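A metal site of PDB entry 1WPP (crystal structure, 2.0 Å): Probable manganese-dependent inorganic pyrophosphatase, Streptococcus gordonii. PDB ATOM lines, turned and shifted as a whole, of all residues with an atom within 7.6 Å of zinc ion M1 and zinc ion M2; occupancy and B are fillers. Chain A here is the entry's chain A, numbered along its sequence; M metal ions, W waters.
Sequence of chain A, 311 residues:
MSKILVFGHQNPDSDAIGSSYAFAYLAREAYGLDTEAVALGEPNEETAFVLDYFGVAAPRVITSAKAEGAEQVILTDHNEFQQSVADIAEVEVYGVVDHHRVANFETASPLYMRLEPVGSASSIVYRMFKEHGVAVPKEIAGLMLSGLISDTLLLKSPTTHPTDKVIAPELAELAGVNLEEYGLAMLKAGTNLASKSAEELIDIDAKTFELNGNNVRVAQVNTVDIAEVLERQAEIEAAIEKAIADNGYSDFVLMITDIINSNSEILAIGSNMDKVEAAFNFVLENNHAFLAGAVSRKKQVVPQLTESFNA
N of Asp 15 lies close to OD2 of Asp 13 (3.5 Å).
The side-chain carboxylate (OD1) of Asp 77 lies close to the backbone NH (N) of Ala 16 (3.3 Å).
The side-chain carboxylate of Asp 15 is in hydrogen-bond range of the side-chain hydroxyl of Ser 122, at 2.9 Å.
O of Asn 11 lies within hydrogen-bond range of ND1 of His 9 (3.5 Å).
O of Asp 77 lies close to ND1 of His 100, at 3.5 Å.
N of Ala 16 sits close to OD2 of Asp 13 (2.9 Å).
The backbone NH of His 9 is in hydrogen-bond range of a ring nitrogen (ND1) of His 78.
OD2 of Asp 98 sits at hydrogen-bond distance from ND1 of His 100 (2.7 Å).
Within 4 Å of zinc ion M1: His 9, Asp 13 and Asp 77.
His 100 touches zinc ion M2 (CE1 to ZN, 3.9 Å).
Five residues have an atom within 4 Å of zinc ion M2: Asp 15, Asp 77, His 99, His 100 and Asp 151.
Zinc ion M1 is bound by the side-chain carboxylate (OD1) of Asp 77 (2.0 Å), the side-chain carboxylate (OD1) of Asp 13 (2.0 Å), water W2 (2.1 Å), a ring nitrogen (NE2) of His 9 (2.1 Å) and the side-chain carboxylate (OD2) of Asp 13 (2.5 Å).
Slightly farther from zinc ion M1 lies water W1 (2.6 Å).
Zinc ion M2 is bound by water W2 (1.9 Å).
OD2 of Asp 151 binds zinc ion M2, 2.0 Å away.
OD2 of Asp 77 binds zinc ion M2.
Zinc ion M2 is bound by the side-chain carboxylate (OD2) of Asp 15 (2.0 Å).
Zinc ion M2 is bound by NE2 of His 99.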
ATOM      1  N   GLY A   8     -12.326  -8.206  14.912  1.00  0.00           N
ATOM      2  CA  GLY A   8     -12.174  -7.948  13.481  1.00  0.00           C
ATOM      3  C   GLY A   8     -12.280  -6.440  13.153  1.00  0.00           C
ATOM      4  O   GLY A   8     -12.338  -5.613  14.076  1.00  0.00           O
ATOM      5  N   HIS A   9     -12.366  -6.114  11.859  1.00  0.00           N
ATOM      6  CA  HIS A   9     -12.299  -4.727  11.385  1.00  0.00           C
ATOM      7  C   HIS A   9     -13.564  -3.957  11.675  1.00  0.00           C
ATOM      8  O   HIS A   9     -14.602  -4.552  12.039  1.00  0.00           O
ATOM      9  CB  HIS A   9     -11.983  -4.650   9.863  1.00  0.00           C
ATOM     10  CG  HIS A   9     -12.778  -5.617   9.013  1.00  0.00           C
ATOM     11  ND1 HIS A   9     -14.056  -5.358   8.581  1.00  0.00           N
ATOM     12  CD2 HIS A   9     -12.446  -6.823   8.489  1.00  0.00           C
ATOM     13  CE1 HIS A   9     -14.489  -6.379   7.835  1.00  0.00           C
ATOM     14  NE2 HIS A   9     -13.522  -7.283   7.763  1.00  0.00           N
ATOM     15  N   GLN A  10     -13.463  -2.635  11.538  1.00  0.00           N
ATOM     16  CA  GLN A  10     -14.617  -1.767  11.458  1.00  0.00           C
ATOM     17  C   GLN A  10     -15.496  -2.209  10.303  1.00  0.00           C
ATOM     18  O   GLN A  10     -15.007  -2.796   9.316  1.00  0.00           O
ATOM     19  CB  GLN A  10     -14.211  -0.299  11.216  1.00  0.00           C
ATOM     20  CG  GLN A  10     -13.343   0.343  12.286  1.00  0.00           C
ATOM     21  CD  GLN A  10     -14.146   0.922  13.436  1.00  0.00           C
ATOM     22  OE1 GLN A  10     -15.361   0.789  13.471  1.00  0.00           O
ATOM     23  NE2 GLN A  10     -13.476   1.554  14.367  1.00  0.00           N
ATOM     24  N   ASN A  11     -16.784  -1.898  10.422  1.00  0.00           N
ATOM     25  CA  ASN A  11     -17.820  -2.447   9.558  1.00  0.00           C
ATOM     26  C   ASN A  11     -17.681  -3.944   9.449  1.00  0.00           C
ATOM     27  O   ASN A  11     -17.378  -4.439   8.373  1.00  0.00           O
ATOM     28  CB  ASN A  11     -17.808  -1.761   8.181  1.00  0.00           C
ATOM     29  CG  ASN A  11     -17.959  -0.248   8.305  1.00  0.00           C
ATOM     30  OD1 ASN A  11     -18.875   0.244   8.983  1.00  0.00           O
ATOM     31  ND2 ASN A  11     -17.051   0.492   7.660  1.00  0.00           N
ATOM     32  N   PRO A  12     -17.793  -4.674  10.556  1.00  0.00           N
ATOM     33  CA  PRO A  12     -17.490  -6.117  10.527  1.00  0.00           C
ATOM     34  C   PRO A  12     -18.335  -6.917   9.511  1.00  0.00           C
ATOM     35  O   PRO A  12     -19.525  -6.642   9.301  1.00  0.00           O
ATOM     36  CB  PRO A  12     -17.745  -6.543  11.970  1.00  0.00           C
ATOM     37  CG  PRO A  12     -18.721  -5.474  12.450  1.00  0.00           C
ATOM     38  CD  PRO A  12     -18.178  -4.221  11.900  1.00  0.00           C
ATOM     39  N   ASP A  13     -17.691  -7.856   8.821  1.00  0.00           N
ATOM     40  CA  ASP A  13     -18.386  -8.756   7.921  1.00  0.00           C
ATOM     41  C   ASP A  13     -18.431 -10.112   8.686  1.00  0.00           C
ATOM     42  O   ASP A  13     -17.914 -10.164   9.792  1.00  0.00           O
ATOM     43  CB  ASP A  13     -17.653  -8.803   6.551  1.00  0.00           C
ATOM     44  CG  ASP A  13     -16.167  -9.151   6.688  1.00  0.00           C
ATOM     45  OD1 ASP A  13     -15.361  -8.884   5.756  1.00  0.00           O
ATOM     46  OD2 ASP A  13     -15.707  -9.745   7.691  1.00  0.00           O
ATOM     47  N   SER A  14     -18.971 -11.202   8.115  1.00  0.00           N
ATOM     48  CA  SER A  14     -19.102 -12.480   8.843  1.00  0.00           C
ATOM     49  C   SER A  14     -17.785 -13.082   9.254  1.00  0.00           C
ATOM     50  O   SER A  14     -17.711 -13.718  10.309  1.00  0.00           O
ATOM     51  CB  SER A  14     -19.842 -13.544   8.018  1.00  0.00           C
ATOM     52  OG  SER A  14     -21.190 -13.134   7.797  1.00  0.00           O
ATOM     53  N   ASP A  15     -16.779 -12.959   8.374  1.00  0.00           N
ATOM     54  CA  ASP A  15     -15.444 -13.457   8.658  1.00  0.00           C
ATOM     55  C   ASP A  15     -14.792 -12.731   9.813  1.00  0.00           C
ATOM     56  O   ASP A  15     -14.117 -13.363  10.614  1.00  0.00           O
ATOM     57  CB  ASP A  15     -14.552 -13.397   7.416  1.00  0.00           C
ATOM     58  CG  ASP A  15     -13.206 -14.061   7.617  1.00  0.00           C
ATOM     59  OD1 ASP A  15     -13.197 -15.151   8.219  1.00  0.00           O
ATOM     60  OD2 ASP A  15     -12.100 -13.554   7.226  1.00  0.00           O
ATOM     61  N   ALA A  16     -14.988 -11.416   9.905  1.00  0.00           N
ATOM     62  CA  ALA A  16     -14.427 -10.606  11.002  1.00  0.00           C
ATOM     63  C   ALA A  16     -14.992 -11.080  12.378  1.00  0.00           C
ATOM     64  O   ALA A  16     -14.233 -11.356  13.346  1.00  0.00           O
ATOM     65  CB  ALA A  16     -14.719  -9.062  10.745  1.00  0.00           C
ATOM     66  N   ILE A  17     -16.311 -11.253  12.446  1.00  0.00           N
ATOM     67  CA  ILE A  17     -16.986 -11.631  13.714  1.00  0.00           C
ATOM     68  C   ILE A  17     -16.646 -13.120  13.966  1.00  0.00           C
ATOM     69  O   ILE A  17     -16.270 -13.511  15.079  1.00  0.00           O
ATOM     70  CB  ILE A  17     -18.546 -11.432  13.559  1.00  0.00           C
ATOM     71  CG1 ILE A  17     -18.951  -9.961  13.457  1.00  0.00           C
ATOM     72  CG2 ILE A  17     -19.385 -12.167  14.645  1.00  0.00           C
ATOM     73  CD1 ILE A  17     -18.659  -9.195  14.587  1.00  0.00           C
ATOM     74  N   SER A  19     -14.129 -15.078  12.859  1.00  0.00           N
ATOM     75  CA  SER A  19     -12.725 -15.282  13.207  1.00  0.00           C
ATOM     76  C   SER A  19     -12.340 -14.822  14.610  1.00  0.00           C
ATOM     77  O   SER A  19     -11.537 -15.506  15.312  1.00  0.00           O
ATOM     78  CB  SER A  19     -11.763 -14.719  12.134  1.00  0.00           C
ATOM     79  OG  SER A  19     -11.797 -13.290  12.102  1.00  0.00           O
ATOM     80  N   THR A  76      -8.065  -9.776  14.162  1.00  0.00           N
ATOM     81  CA  THR A  76      -8.283 -10.894  13.229  1.00  0.00           C
ATOM     82  C   THR A  76      -8.901 -10.327  11.993  1.00  0.00           C
ATOM     83  O   THR A  76      -9.546  -9.274  12.078  1.00  0.00           O
ATOM     84  CB  THR A  76      -9.147 -12.041  13.796  1.00  0.00           C
ATOM     85  OG1 THR A  76     -10.518 -11.622  14.019  1.00  0.00           O
ATOM     86  CG2 THR A  76      -8.610 -12.560  15.192  1.00  0.00           C
ATOM     87  N   ASP A  77      -8.665 -10.956  10.824  1.00  0.00           N
ATOM     88  CA  ASP A  77      -9.244 -10.487   9.547  1.00  0.00           C
ATOM     89  C   ASP A  77      -8.871  -9.022   9.174  1.00  0.00           C
ATOM     90  O   ASP A  77      -9.477  -8.435   8.272  1.00  0.00           O
ATOM     91  CB  ASP A  77     -10.788 -10.657   9.561  1.00  0.00           C
ATOM     92  CG  ASP A  77     -11.435 -10.566   8.169  1.00  0.00           C
ATOM     93  OD1 ASP A  77     -12.588 -10.060   8.096  1.00  0.00           O
ATOM     94  OD2 ASP A  77     -10.903 -11.000   7.110  1.00  0.00           O
ATOM     95  N   HIS A  78      -7.840  -8.469   9.774  1.00  0.00           N
ATOM     96  CA  HIS A  78      -7.336  -7.141   9.344  1.00  0.00           C
ATOM     97  C   HIS A  78      -6.001  -6.846  10.025  1.00  0.00           C
ATOM     98  O   HIS A  78      -5.640  -7.496  11.033  1.00  0.00           O
ATOM     99  CB  HIS A  78      -8.335  -6.009   9.677  1.00  0.00           C
ATOM    100  CG  HIS A  78      -8.405  -5.664  11.129  1.00  0.00           C
ATOM    101  ND1 HIS A  78      -8.919  -6.522  12.077  1.00  0.00           N
ATOM    102  CD2 HIS A  78      -8.037  -4.534  11.803  1.00  0.00           C
ATOM    103  CE1 HIS A  78      -8.877  -5.941  13.270  1.00  0.00           C
ATOM    104  NE2 HIS A  78      -8.346  -4.739  13.129  1.00  0.00           N
ATOM    105  N   GLN A  83      -8.483   0.432   9.594  1.00  0.00           N
ATOM    106  CA  GLN A  83      -9.583  -0.526   9.681  1.00  0.00           C
ATOM    107  C   GLN A  83      -9.824  -0.970  11.101  1.00  0.00           C
ATOM    108  O   GLN A  83     -10.754  -1.755  11.344  1.00  0.00           O
ATOM    109  CB  GLN A  83      -9.309  -1.775   8.832  1.00  0.00           C
ATOM    110  CG  GLN A  83      -9.219  -1.460   7.333  1.00  0.00           C
ATOM    111  CD  GLN A  83      -8.797  -2.690   6.528  1.00  0.00           C
ATOM    112  OE1 GLN A  83      -8.636  -3.759   7.101  1.00  0.00           O
ATOM    113  NE2 GLN A  83      -8.627  -2.550   5.235  1.00  0.00           N
ATOM    114  N   ASP A  98      -4.622 -12.965   9.860  1.00  0.00           N
ATOM    115  CA  ASP A  98      -5.289 -12.286   8.766  1.00  0.00           C
ATOM    116  C   ASP A  98      -5.015 -12.980   7.431  1.00  0.00           C
ATOM    117  O   ASP A  98      -4.189 -13.896   7.388  1.00  0.00           O
ATOM    118  CB  ASP A  98      -4.821 -10.815   8.765  1.00  0.00           C
ATOM    119  CG  ASP A  98      -5.667  -9.937   7.881  1.00  0.00           C
ATOM    120  OD1 ASP A  98      -5.181  -8.840   7.517  1.00  0.00           O
ATOM    121  OD2 ASP A  98      -6.813 -10.268   7.497  1.00  0.00           O
ATOM    122  N   HIS A  99      -5.702 -12.531   6.359  1.00  0.00           N
ATOM    123  CA  HIS A  99      -5.582 -13.022   4.986  1.00  0.00           C
ATOM    124  C   HIS A  99      -5.527 -11.868   3.928  1.00  0.00           C
ATOM    125  O   HIS A  99      -5.818 -12.065   2.749  1.00  0.00           O
ATOM    126  CB  HIS A  99      -6.683 -14.040   4.668  1.00  0.00           C
ATOM    127  CG  HIS A  99      -8.084 -13.466   4.584  1.00  0.00           C
ATOM    128  ND1 HIS A  99      -8.820 -13.479   3.411  1.00  0.00           N
ATOM    129  CD2 HIS A  99      -8.914 -12.970   5.529  1.00  0.00           C
ATOM    130  CE1 HIS A  99     -10.014 -12.953   3.629  1.00  0.00           C
ATOM    131  NE2 HIS A  99     -10.105 -12.650   4.920  1.00  0.00           N
ATOM    132  N   HIS A 100      -5.167 -10.683   4.378  1.00  0.00           N
ATOM    133  CA  HIS A 100      -5.070  -9.512   3.471  1.00  0.00           C
ATOM    134  C   HIS A 100      -3.628  -9.094   3.291  1.00  0.00           C
ATOM    135  O   HIS A 100      -2.731  -9.564   3.999  1.00  0.00           O
ATOM    136  CB  HIS A 100      -5.910  -8.353   4.037  1.00  0.00           C
ATOM    137  CG  HIS A 100      -7.362  -8.677   4.118  1.00  0.00           C
ATOM    138  ND1 HIS A 100      -7.923  -9.240   5.245  1.00  0.00           N
ATOM    139  CD2 HIS A 100      -8.378  -8.554   3.214  1.00  0.00           C
ATOM    140  CE1 HIS A 100      -9.214  -9.428   5.028  1.00  0.00           C
ATOM    141  NE2 HIS A 100      -9.522  -8.998   3.813  1.00  0.00           N
ATOM    142  N   VAL A 118      -5.223 -17.037   1.926  1.00  0.00           N
ATOM    143  CA  VAL A 118      -6.290 -18.017   1.711  1.00  0.00           C
ATOM    144  C   VAL A 118      -7.613 -17.266   1.733  1.00  0.00           C
ATOM    145  O   VAL A 118      -7.629 -16.034   1.712  1.00  0.00           O
ATOM    146  CB  VAL A 118      -6.266 -19.170   2.783  1.00  0.00           C
ATOM    147  CG1 VAL A 118      -4.947 -19.975   2.700  1.00  0.00           C
ATOM    148  CG2 VAL A 118      -6.457 -18.631   4.225  1.00  0.00           C
ATOM    149  N   GLY A 119      -8.730 -17.993   1.779  1.00  0.00           N
ATOM    150  CA  GLY A 119     -10.035 -17.407   1.491  1.00  0.00           C
ATOM    151  C   GLY A 119     -10.615 -16.548   2.611  1.00  0.00           C
ATOM    152  O   GLY A 119     -11.418 -15.676   2.334  1.00  0.00           O
ATOM    153  N   SER A 120     -10.189 -16.783   3.852  1.00  0.00           N
ATOM    154  CA  SER A 120     -10.779 -16.075   4.987  1.00  0.00           C
ATOM    155  C   SER A 120      -9.862 -16.264   6.173  1.00  0.00           C
ATOM    156  O   SER A 120      -9.078 -17.242   6.243  1.00  0.00           O
ATOM    157  CB  SER A 120     -12.150 -16.666   5.371  1.00  0.00           C
ATOM    158  OG  SER A 120     -11.964 -18.011   5.883  1.00  0.00           O
ATOM    159  N   ALA A 121      -9.989 -15.371   7.160  1.00  0.00           N
ATOM    160  CA  ALA A 121      -9.276 -15.514   8.411  1.00  0.00           C
ATOM    161  C   ALA A 121      -9.812 -16.706   9.198  1.00  0.00           C
ATOM    162  O   ALA A 121      -9.052 -17.369   9.918  1.00  0.00           O
ATOM    163  CB  ALA A 121      -9.371 -14.233   9.254  1.00  0.00           C
ATOM    164  N   SER A 122     -11.082 -17.014   9.016  1.00  0.00           N
ATOM    165  CA  SER A 122     -11.672 -18.099   9.777  1.00  0.00           C
ATOM    166  C   SER A 122     -11.033 -19.449   9.379  1.00  0.00           C
ATOM    167  O   SER A 122     -10.923 -20.367  10.219  1.00  0.00           O
ATOM    168  CB  SER A 122     -13.184 -18.150   9.557  1.00  0.00           C
ATOM    169  OG  SER A 122     -13.861 -17.132  10.252  1.00  0.00           O
ATOM    170  N   GLY A 147     -17.783 -17.642   8.006  1.00  0.00           N
ATOM    171  CA  GLY A 147     -16.753 -16.710   7.608  1.00  0.00           C
ATOM    172  C   GLY A 147     -16.157 -17.044   6.253  1.00  0.00           C
ATOM    173  O   GLY A 147     -16.026 -16.162   5.373  1.00  0.00           O
ATOM    174  N   LEU A 148     -15.806 -18.318   6.085  1.00  0.00           N
ATOM    175  CA  LEU A 148     -15.275 -18.845   4.840  1.00  0.00           C
ATOM    176  C   LEU A 148     -16.264 -18.770   3.691  1.00  0.00           C
ATOM    177  O   LEU A 148     -15.903 -18.307   2.583  1.00  0.00           O
ATOM    178  CB  LEU A 148     -14.743 -20.273   5.039  1.00  0.00           C
ATOM    179  CG  LEU A 148     -14.344 -21.058   3.751  1.00  0.00           C
ATOM    180  CD1 LEU A 148     -13.218 -20.336   2.900  1.00  0.00           C
ATOM    181  CD2 LEU A 148     -14.031 -22.535   4.088  1.00  0.00           C
ATOM    182  N   SER A 150     -18.854 -16.680   3.440  1.00  0.00           N
ATOM    183  CA  SER A 150     -19.090 -15.256   3.151  1.00  0.00           C
ATOM    184  C   SER A 150     -17.987 -14.608   2.325  1.00  0.00           C
ATOM    185  O   SER A 150     -18.276 -13.935   1.282  1.00  0.00           O
ATOM    186  CB  SER A 150     -19.252 -14.489   4.478  1.00  0.00           C
ATOM    187  OG  SER A 150     -19.220 -13.101   4.312  1.00  0.00           O
ATOM    188  N   ASP A 151     -16.728 -14.808   2.728  1.00  0.00           N
ATOM    189  CA  ASP A 151     -15.577 -14.188   2.044  1.00  0.00           C
ATOM    190  C   ASP A 151     -15.363 -14.721   0.594  1.00  0.00           C
ATOM    191  O   ASP A 151     -14.851 -13.999  -0.268  1.00  0.00           O
ATOM    192  CB  ASP A 151     -14.262 -14.341   2.834  1.00  0.00           C
ATOM    193  CG  ASP A 151     -13.988 -13.204   3.804  1.00  0.00           C
ATOM    194  OD1 ASP A 151     -14.814 -12.228   3.926  1.00  0.00           O
ATOM    195  OD2 ASP A 151     -12.942 -13.228   4.521  1.00  0.00           O
ATOM    196  N   ASP A 205     -19.944  -1.853   1.490  1.00  0.00           N
ATOM    197  CA  ASP A 205     -18.632  -2.462   1.398  1.00  0.00           C
ATOM    198  C   ASP A 205     -17.852  -1.755   0.286  1.00  0.00           C
ATOM    199  O   ASP A 205     -17.858  -2.185  -0.854  1.00  0.00           O
ATOM    200  CB  ASP A 205     -18.776  -3.951   1.128  1.00  0.00           C
ATOM    201  CG  ASP A 205     -17.473  -4.711   1.147  1.00  0.00           C
ATOM    202  OD1 ASP A 205     -16.373  -4.113   1.161  1.00  0.00           O
ATOM    203  OD2 ASP A 205     -17.453  -5.959   1.141  1.00  0.00           O
ATOM    204  N   LYS A 298     -10.808  -7.689  -5.012  1.00  0.00           N
ATOM    205  CA  LYS A 298      -9.390  -7.529  -4.974  1.00  0.00           C
ATOM    206  C   LYS A 298      -8.709  -8.356  -6.063  1.00  0.00           C
ATOM    207  O   LYS A 298      -7.615  -8.031  -6.442  1.00  0.00           O
ATOM    208  CB  LYS A 298      -8.825  -7.839  -3.552  1.00  0.00           C
ATOM    209  CG  LYS A 298      -8.407  -9.256  -3.293  1.00  0.00           C
ATOM    210  CD  LYS A 298      -7.988  -9.353  -1.806  1.00  0.00           C
ATOM    211  CE  LYS A 298      -8.378 -10.643  -1.218  1.00  0.00           C
ATOM    212  NZ  LYS A 298      -9.689 -10.634  -0.429  1.00  0.00           N
HETATM  213 ZN    ZN M   1     -13.518  -9.052   6.618  1.00  0.00          ZN
HETATM  214 ZN    ZN M   2     -11.937 -12.112   5.812  1.00  0.00          ZN
HETATM  215  O   HOH W   1     -12.156  -7.491   5.001  1.00  0.00           O
HETATM  216  O   HOH W   2     -13.090 -10.632   5.367  1.00  0.00           O
